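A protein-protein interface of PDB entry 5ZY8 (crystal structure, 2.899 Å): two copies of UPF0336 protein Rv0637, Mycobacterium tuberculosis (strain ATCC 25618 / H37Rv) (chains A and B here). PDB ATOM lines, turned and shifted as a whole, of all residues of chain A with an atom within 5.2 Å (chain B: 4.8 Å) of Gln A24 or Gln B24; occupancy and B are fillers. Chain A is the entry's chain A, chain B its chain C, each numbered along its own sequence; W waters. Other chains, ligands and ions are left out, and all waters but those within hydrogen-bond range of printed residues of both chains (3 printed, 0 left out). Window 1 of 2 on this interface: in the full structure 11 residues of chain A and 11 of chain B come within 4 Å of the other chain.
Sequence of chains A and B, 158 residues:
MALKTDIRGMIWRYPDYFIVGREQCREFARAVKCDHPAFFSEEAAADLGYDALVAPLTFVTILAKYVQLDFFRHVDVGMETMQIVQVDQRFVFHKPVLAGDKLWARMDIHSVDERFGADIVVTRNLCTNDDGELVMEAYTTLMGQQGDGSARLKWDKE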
ATOM      1  N   ILE A  19      21.214 -23.908 -28.812  1.00  0.00           N
ATOM      2  CA  ILE A  19      20.272 -23.818 -27.693  1.00  0.00           C
ATOM      3  C   ILE A  19      20.384 -22.450 -27.035  1.00  0.00           C
ATOM      4  O   ILE A  19      21.484 -22.008 -26.679  1.00  0.00           O
ATOM      5  CB  ILE A  19      20.488 -24.945 -26.664  1.00  0.00           C
ATOM      6  CG1 ILE A  19      20.232 -26.306 -27.313  1.00  0.00           C
ATOM      7  CG2 ILE A  19      19.609 -24.717 -25.448  1.00  0.00           C
ATOM      8  CD1 ILE A  19      18.784 -26.529 -27.649  1.00  0.00           C
ATOM      9  N   GLY A  21      20.447 -20.496 -24.083  1.00  0.00           N
ATOM     10  CA  GLY A  21      20.725 -20.915 -22.716  1.00  0.00           C
ATOM     11  C   GLY A  21      20.229 -19.902 -21.699  1.00  0.00           C
ATOM     12  O   GLY A  21      20.463 -18.699 -21.837  1.00  0.00           O
ATOM     13  N   ARG A  22      19.530 -20.401 -20.675  1.00  0.00           N
ATOM     14  CA  ARG A  22      18.931 -19.534 -19.664  1.00  0.00           C
ATOM     15  C   ARG A  22      19.987 -18.672 -18.971  1.00  0.00           C
ATOM     16  O   ARG A  22      19.934 -17.437 -19.026  1.00  0.00           O
ATOM     17  CB  ARG A  22      18.170 -20.390 -18.656  1.00  0.00           C
ATOM     18  CG  ARG A  22      17.444 -19.629 -17.566  1.00  0.00           C
ATOM     19  CD  ARG A  22      16.826 -20.644 -16.631  1.00  0.00           C
ATOM     20  NE  ARG A  22      16.060 -20.111 -15.508  1.00  0.00           N
ATOM     21  CZ  ARG A  22      16.481 -20.159 -14.244  1.00  0.00           C
ATOM     22  NH1 ARG A  22      17.672 -20.671 -13.961  1.00  0.00           N
ATOM     23  NH2 ARG A  22      15.721 -19.706 -13.262  1.00  0.00           N
ATOM     24  N   GLU A  23      20.958 -19.309 -18.311  1.00  0.00           N
ATOM     25  CA  GLU A  23      21.920 -18.544 -17.525  1.00  0.00           C
ATOM     26  C   GLU A  23      22.734 -17.603 -18.410  1.00  0.00           C
ATOM     27  O   GLU A  23      23.097 -16.498 -17.986  1.00  0.00           O
ATOM     28  CB  GLU A  23      22.848 -19.493 -16.758  1.00  0.00           C
ATOM     29  CG  GLU A  23      22.150 -20.682 -16.086  1.00  0.00           C
ATOM     30  CD  GLU A  23      21.007 -20.299 -15.143  1.00  0.00           C
ATOM     31  OE1 GLU A  23      21.124 -19.273 -14.443  1.00  0.00           O
ATOM     32  OE2 GLU A  23      19.989 -21.022 -15.098  1.00  0.00           O
ATOM     33  N   GLN A  24      23.021 -18.012 -19.647  1.00  0.00           N
ATOM     34  CA  GLN A  24      23.807 -17.163 -20.537  1.00  0.00           C
ATOM     35  C   GLN A  24      23.011 -15.925 -20.981  1.00  0.00           C
ATOM     36  O   GLN A  24      23.533 -14.805 -20.962  1.00  0.00           O
ATOM     37  CB  GLN A  24      24.269 -17.996 -21.724  1.00  0.00           C
ATOM     38  CG  GLN A  24      25.286 -17.367 -22.617  1.00  0.00           C
ATOM     39  CD  GLN A  24      25.657 -18.300 -23.750  1.00  0.00           C
ATOM     40  OE1 GLN A  24      24.872 -19.183 -24.121  1.00  0.00           O
ATOM     41  NE2 GLN A  24      26.864 -18.134 -24.294  1.00  0.00           N
ATOM     42  N   CYS A  25      21.737 -16.103 -21.348  1.00  0.00           N
ATOM     43  CA  CYS A  25      20.853 -14.968 -21.592  1.00  0.00           C
ATOM     44  C   CYS A  25      20.902 -13.994 -20.434  1.00  0.00           C
ATOM     45  O   CYS A  25      21.052 -12.782 -20.619  1.00  0.00           O
ATOM     46  CB  CYS A  25      19.415 -15.445 -21.745  1.00  0.00           C
ATOM     47  SG  CYS A  25      19.023 -16.166 -23.275  1.00  0.00           S
ATOM     48  N   ARG A  26      20.723 -14.517 -19.224  1.00  0.00           N
ATOM     49  CA  ARG A  26      20.743 -13.674 -18.042  1.00  0.00           C
ATOM     50  C   ARG A  26      22.046 -12.896 -17.949  1.00  0.00           C
ATOM     51  O   ARG A  26      22.034 -11.686 -17.693  1.00  0.00           O
ATOM     52  CB  ARG A  26      20.563 -14.541 -16.803  1.00  0.00           C
ATOM     53  CG  ARG A  26      19.169 -15.075 -16.535  1.00  0.00           C
ATOM     54  CD  ARG A  26      19.203 -15.667 -15.142  1.00  0.00           C
ATOM     55  NE  ARG A  26      17.896 -15.906 -14.561  1.00  0.00           N
ATOM     56  CZ  ARG A  26      17.671 -16.837 -13.645  1.00  0.00           C
ATOM     57  NH1 ARG A  26      18.662 -17.607 -13.222  1.00  0.00           N
ATOM     58  NH2 ARG A  26      16.461 -16.986 -13.146  1.00  0.00           N
ATOM     59  N   GLU A  27      23.181 -13.564 -18.186  1.00  0.00           N
ATOM     60  CA  GLU A  27      24.466 -12.883 -18.082  1.00  0.00           C
ATOM     61  C   GLU A  27      24.646 -11.885 -19.221  1.00  0.00           C
ATOM     62  O   GLU A  27      25.080 -10.748 -18.999  1.00  0.00           O
ATOM     63  CB  GLU A  27      25.598 -13.910 -18.067  1.00  0.00           C
ATOM     64  CG  GLU A  27      25.788 -14.681 -16.746  1.00  0.00           C
ATOM     65  CD  GLU A  27      26.107 -13.791 -15.554  1.00  0.00           C
ATOM     66  OE1 GLU A  27      26.677 -12.697 -15.763  1.00  0.00           O
ATOM     67  OE2 GLU A  27      25.815 -14.189 -14.400  1.00  0.00           O
ATOM     68  N   PHE A  28      24.272 -12.285 -20.442  1.00  0.00           N
ATOM     69  CA  PHE A  28      24.281 -11.374 -21.586  1.00  0.00           C
ATOM     70  C   PHE A  28      23.404 -10.152 -21.327  1.00  0.00           C
ATOM     71  O   PHE A  28      23.815  -9.013 -21.576  1.00  0.00           O
ATOM     72  CB  PHE A  28      23.808 -12.129 -22.831  1.00  0.00           C
ATOM     73  CG  PHE A  28      24.067 -11.416 -24.126  1.00  0.00           C
ATOM     74  CD1 PHE A  28      23.189 -10.430 -24.581  1.00  0.00           C
ATOM     75  CD2 PHE A  28      25.170 -11.732 -24.904  1.00  0.00           C
ATOM     76  CE1 PHE A  28      23.406  -9.771 -25.782  1.00  0.00           C
ATOM     77  CE2 PHE A  28      25.390 -11.067 -26.114  1.00  0.00           C
ATOM     78  CZ  PHE A  28      24.503 -10.087 -26.549  1.00  0.00           C
ATOM     79  N   ALA A  29      22.189 -10.374 -20.826  1.00  0.00           N
ATOM     80  CA  ALA A  29      21.290  -9.262 -20.541  1.00  0.00           C
ATOM     81  C   ALA A  29      21.948  -8.263 -19.600  1.00  0.00           C
ATOM     82  O   ALA A  29      21.891  -7.047 -19.821  1.00  0.00           O
ATOM     83  CB  ALA A  29      19.983  -9.786 -19.949  1.00  0.00           C
ATOM     84  N   PHE A  59      20.789 -11.086 -28.690  1.00  0.00           N
ATOM     85  CA  PHE A  59      21.445 -12.307 -28.224  1.00  0.00           C
ATOM     86  C   PHE A  59      21.988 -13.147 -29.375  1.00  0.00           C
ATOM     87  O   PHE A  59      23.101 -13.684 -29.291  1.00  0.00           O
ATOM     88  CB  PHE A  59      20.478 -13.142 -27.407  1.00  0.00           C
ATOM     89  CG  PHE A  59      21.142 -14.257 -26.669  1.00  0.00           C
ATOM     90  CD1 PHE A  59      21.996 -13.986 -25.609  1.00  0.00           C
ATOM     91  CD2 PHE A  59      20.964 -15.572 -27.067  1.00  0.00           C
ATOM     92  CE1 PHE A  59      22.618 -15.006 -24.931  1.00  0.00           C
ATOM     93  CE2 PHE A  59      21.589 -16.586 -26.407  1.00  0.00           C
ATOM     94  CZ  PHE A  59      22.419 -16.304 -25.331  1.00  0.00           C
ATOM     95  N   ILE A  62      25.559 -13.923 -31.056  1.00  0.00           N
ATOM     96  CA  ILE A  62      26.473 -15.021 -30.759  1.00  0.00           C
ATOM     97  C   ILE A  62      26.371 -16.086 -31.843  1.00  0.00           C
ATOM     98  O   ILE A  62      27.383 -16.542 -32.401  1.00  0.00           O
ATOM     99  CB  ILE A  62      26.165 -15.598 -29.366  1.00  0.00           C
ATOM    100  CG1 ILE A  62      26.588 -14.610 -28.283  1.00  0.00           C
ATOM    101  CG2 ILE A  62      26.845 -16.942 -29.177  1.00  0.00           C
ATOM    102  CD1 ILE A  62      25.861 -14.771 -26.984  1.00  0.00           C
ATOM    103  N   GLY B  21      23.941 -24.953 -19.219  1.00  0.00           N
ATOM    104  CA  GLY B  21      23.611 -24.591 -20.583  1.00  0.00           C
ATOM    105  C   GLY B  21      24.616 -25.124 -21.584  1.00  0.00           C
ATOM    106  O   GLY B  21      25.826 -25.000 -21.387  1.00  0.00           O
ATOM    107  N   ARG B  22      24.099 -25.698 -22.680  1.00  0.00           N
ATOM    108  CA  ARG B  22      24.943 -26.350 -23.688  1.00  0.00           C
ATOM    109  C   ARG B  22      25.997 -25.402 -24.255  1.00  0.00           C
ATOM    110  O   ARG B  22      27.202 -25.623 -24.073  1.00  0.00           O
ATOM    111  CB  ARG B  22      24.068 -26.914 -24.817  1.00  0.00           C
ATOM    112  CG  ARG B  22      24.827 -27.616 -25.949  1.00  0.00           C
ATOM    113  CD  ARG B  22      23.846 -28.075 -27.024  1.00  0.00           C
ATOM    114  NE  ARG B  22      24.471 -28.747 -28.166  1.00  0.00           N
ATOM    115  CZ  ARG B  22      24.471 -28.278 -29.415  1.00  0.00           C
ATOM    116  NH1 ARG B  22      23.886 -27.124 -29.689  1.00  0.00           N
ATOM    117  NH2 ARG B  22      25.048 -28.962 -30.392  1.00  0.00           N
ATOM    118  N   GLU B  23      25.562 -24.324 -24.929  1.00  0.00           N
ATOM    119  CA  GLU B  23      26.530 -23.447 -25.589  1.00  0.00           C
ATOM    120  C   GLU B  23      27.478 -22.827 -24.580  1.00  0.00           C
ATOM    121  O   GLU B  23      28.671 -22.642 -24.865  1.00  0.00           O
ATOM    122  CB  GLU B  23      25.840 -22.318 -26.369  1.00  0.00           C
ATOM    123  CG  GLU B  23      24.650 -22.667 -27.274  1.00  0.00           C
ATOM    124  CD  GLU B  23      24.945 -23.768 -28.291  1.00  0.00           C
ATOM    125  OE1 GLU B  23      23.996 -24.520 -28.625  1.00  0.00           O
ATOM    126  OE2 GLU B  23      26.098 -23.855 -28.784  1.00  0.00           O
ATOM    127  N   GLN B  24      26.977 -22.539 -23.383  1.00  0.00           N
ATOM    128  CA  GLN B  24      27.818 -21.909 -22.382  1.00  0.00           C
ATOM    129  C   GLN B  24      28.911 -22.862 -21.927  1.00  0.00           C
ATOM    130  O   GLN B  24      30.067 -22.453 -21.770  1.00  0.00           O
ATOM    131  CB  GLN B  24      26.951 -21.441 -21.216  1.00  0.00           C
ATOM    132  CG  GLN B  24      27.682 -20.624 -20.187  1.00  0.00           C
ATOM    133  CD  GLN B  24      26.773 -20.174 -19.069  1.00  0.00           C
ATOM    134  OE1 GLN B  24      25.708 -20.760 -18.835  1.00  0.00           O
ATOM    135  NE2 GLN B  24      27.202 -19.152 -18.342  1.00  0.00           N
ATOM    136  N   CYS B  25      28.557 -24.138 -21.720  1.00  0.00           N
ATOM    137  CA  CYS B  25      29.544 -25.177 -21.421  1.00  0.00           C
ATOM    138  C   CYS B  25      30.639 -25.236 -22.472  1.00  0.00           C
ATOM    139  O   CYS B  25      31.831 -25.253 -22.142  1.00  0.00           O
ATOM    140  CB  CYS B  25      28.867 -26.540 -21.310  1.00  0.00           C
ATOM    141  SG  CYS B  25      28.057 -26.804 -19.766  1.00  0.00           S
ATOM    142  N   ARG B  26      30.252 -25.317 -23.746  1.00  0.00           N
ATOM    143  CA  ARG B  26      31.248 -25.400 -24.807  1.00  0.00           C
ATOM    144  C   ARG B  26      32.192 -24.196 -24.786  1.00  0.00           C
ATOM    145  O   ARG B  26      33.406 -24.355 -24.962  1.00  0.00           O
ATOM    146  CB  ARG B  26      30.559 -25.584 -26.157  1.00  0.00           C
ATOM    147  CG  ARG B  26      29.986 -26.998 -26.267  1.00  0.00           C
ATOM    148  CD  ARG B  26      29.652 -27.459 -27.686  1.00  0.00           C
ATOM    149  NE  ARG B  26      28.680 -26.640 -28.405  1.00  0.00           N
ATOM    150  CZ  ARG B  26      27.968 -27.092 -29.434  1.00  0.00           C
ATOM    151  NH1 ARG B  26      28.126 -28.347 -29.839  1.00  0.00           N
ATOM    152  NH2 ARG B  26      27.096 -26.303 -30.049  1.00  0.00           N
ATOM    153  N   GLU B  27      31.664 -22.989 -24.547  1.00  0.00           N
ATOM    154  CA  GLU B  27      32.533 -21.815 -24.452  1.00  0.00           C
ATOM    155  C   GLU B  27      33.429 -21.887 -23.217  1.00  0.00           C
ATOM    156  O   GLU B  27      34.614 -21.540 -23.280  1.00  0.00           O
ATOM    157  CB  GLU B  27      31.701 -20.524 -24.426  1.00  0.00           C
ATOM    158  CG  GLU B  27      31.194 -20.064 -25.779  1.00  0.00           C
ATOM    159  CD  GLU B  27      32.327 -19.778 -26.751  1.00  0.00           C
ATOM    160  OE1 GLU B  27      33.435 -19.396 -26.303  1.00  0.00           O
ATOM    161  OE2 GLU B  27      32.116 -19.949 -27.968  1.00  0.00           O
ATOM    162  N   PHE B  28      32.875 -22.327 -22.083  1.00  0.00           N
ATOM    163  CA  PHE B  28      33.690 -22.544 -20.893  1.00  0.00           C
ATOM    164  C   PHE B  28      34.788 -23.569 -21.176  1.00  0.00           C
ATOM    165  O   PHE B  28      35.951 -23.371 -20.802  1.00  0.00           O
ATOM    166  CB  PHE B  28      32.797 -22.998 -19.731  1.00  0.00           C
ATOM    167  CG  PHE B  28      33.427 -22.844 -18.365  1.00  0.00           C
ATOM    168  CD1 PHE B  28      34.339 -23.785 -17.885  1.00  0.00           C
ATOM    169  CD2 PHE B  28      33.072 -21.786 -17.542  1.00  0.00           C
ATOM    170  CE1 PHE B  28      34.913 -23.647 -16.628  1.00  0.00           C
ATOM    171  CE2 PHE B  28      33.639 -21.645 -16.285  1.00  0.00           C
ATOM    172  CZ  PHE B  28      34.562 -22.578 -15.825  1.00  0.00           C
ATOM    173  N   PHE B  59      32.974 -26.236 -14.159  1.00  0.00           N
ATOM    174  CA  PHE B  59      31.911 -25.345 -14.627  1.00  0.00           C
ATOM    175  C   PHE B  59      31.090 -24.796 -13.475  1.00  0.00           C
ATOM    176  O   PHE B  59      30.723 -23.612 -13.470  1.00  0.00           O
ATOM    177  CB  PHE B  59      30.995 -26.083 -15.608  1.00  0.00           C
ATOM    178  CG  PHE B  59      30.006 -25.193 -16.335  1.00  0.00           C
ATOM    179  CD1 PHE B  59      30.430 -24.250 -17.266  1.00  0.00           C
ATOM    180  CD2 PHE B  59      28.648 -25.315 -16.097  1.00  0.00           C
ATOM    181  CE1 PHE B  59      29.503 -23.441 -17.951  1.00  0.00           C
ATOM    182  CE2 PHE B  59      27.722 -24.518 -16.763  1.00  0.00           C
ATOM    183  CZ  PHE B  59      28.148 -23.576 -17.694  1.00  0.00           C
ATOM    184  N   ILE B  62      30.562 -21.383 -11.387  1.00  0.00           N
ATOM    185  CA  ILE B  62      29.605 -20.306 -11.603  1.00  0.00           C
ATOM    186  C   ILE B  62      28.444 -20.423 -10.622  1.00  0.00           C
ATOM    187  O   ILE B  62      28.054 -19.448  -9.971  1.00  0.00           O
ATOM    188  CB  ILE B  62      29.118 -20.294 -13.063  1.00  0.00           C
ATOM    189  CG1 ILE B  62      30.241 -19.829 -13.987  1.00  0.00           C
ATOM    190  CG2 ILE B  62      27.918 -19.377 -13.209  1.00  0.00           C
ATOM    191  CD1 ILE B  62      30.053 -20.249 -15.423  1.00  0.00           C
HETATM  192  O   HOH W   1      23.548 -21.111 -20.560  1.00  0.00           O
HETATM  193  O   HOH W   2      24.211 -21.828 -22.984  1.00  0.00           O
HETATM  194  O   HOH W   3      22.697 -23.513 -24.455  1.00  0.00           O
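Of the printed residues of chain B, Ile A19 touches Glu B23 (2.9 Å).
Printed residues of chain B within 4 Å of Glu A23: Gln B24.
Gln A24 touches two residues of chain B.
Cys A25 touches none of the printed residues of chain B.
Of the printed residues of chain A, Glu B23 touches Ile A19 (2.9 Å) and Gln A24 (3.98 Å).
Of chain A, only Glu A23 and Gln A24 come within 4 Å of Gln B24.
Phe B59 touches none of the printed residues of chain A.
OE1 of Glu B23 sits at hydrogen-bond distance from N of Ile A19 (2.9 Å).
Glu A23 touches Gln B24, and with the chains exchanged Gln A24 touches Glu B23.
Gln A24 touches its own counterpart, Gln B24.
Water W1 bridges the side-chain amide oxygen of Gln B24 (2.8 Å) and the backbone NH of Gln A24 (3.3 Å).
Water W2 lies within hydrogen-bond range of the backbone NH (N) of Gln B24 (2.9 Å), the side-chain amide oxygen (OE1) of Gln A24 (3.0 Å) and the backbone NH (N) of Glu B23 (3.4 Å).
Water W3 lies within hydrogen-bond range of the backbone carbonyl oxygen of Ile A19, the backbone NH of Glu B23 and the backbone NH of Arg B22.
Glu A23 touches Gln B24 (CB to OE1, 3.8 Å).
Gln A24 touches Glu B23.
OE1 of Gln B24 touches N of Gln A24 (3.9 Å).
NH1 of Arg A22 is in salt-bridge range of OE2 of Glu A23, at 2.6 Å.
The side-chain carboxylate of Glu A23 lies within salt-bridge range of the guanidinium group of Arg A26, at 3.2 Å.
NH1 of Arg B22 is in salt-bridge range of OE1 of Glu B23, 2.8 Å away.
The guanidinium group (NH2) of Arg B26 lies within salt-bridge range of the side-chain carboxylate (OE2) of Glu B23 (2.9 Å).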
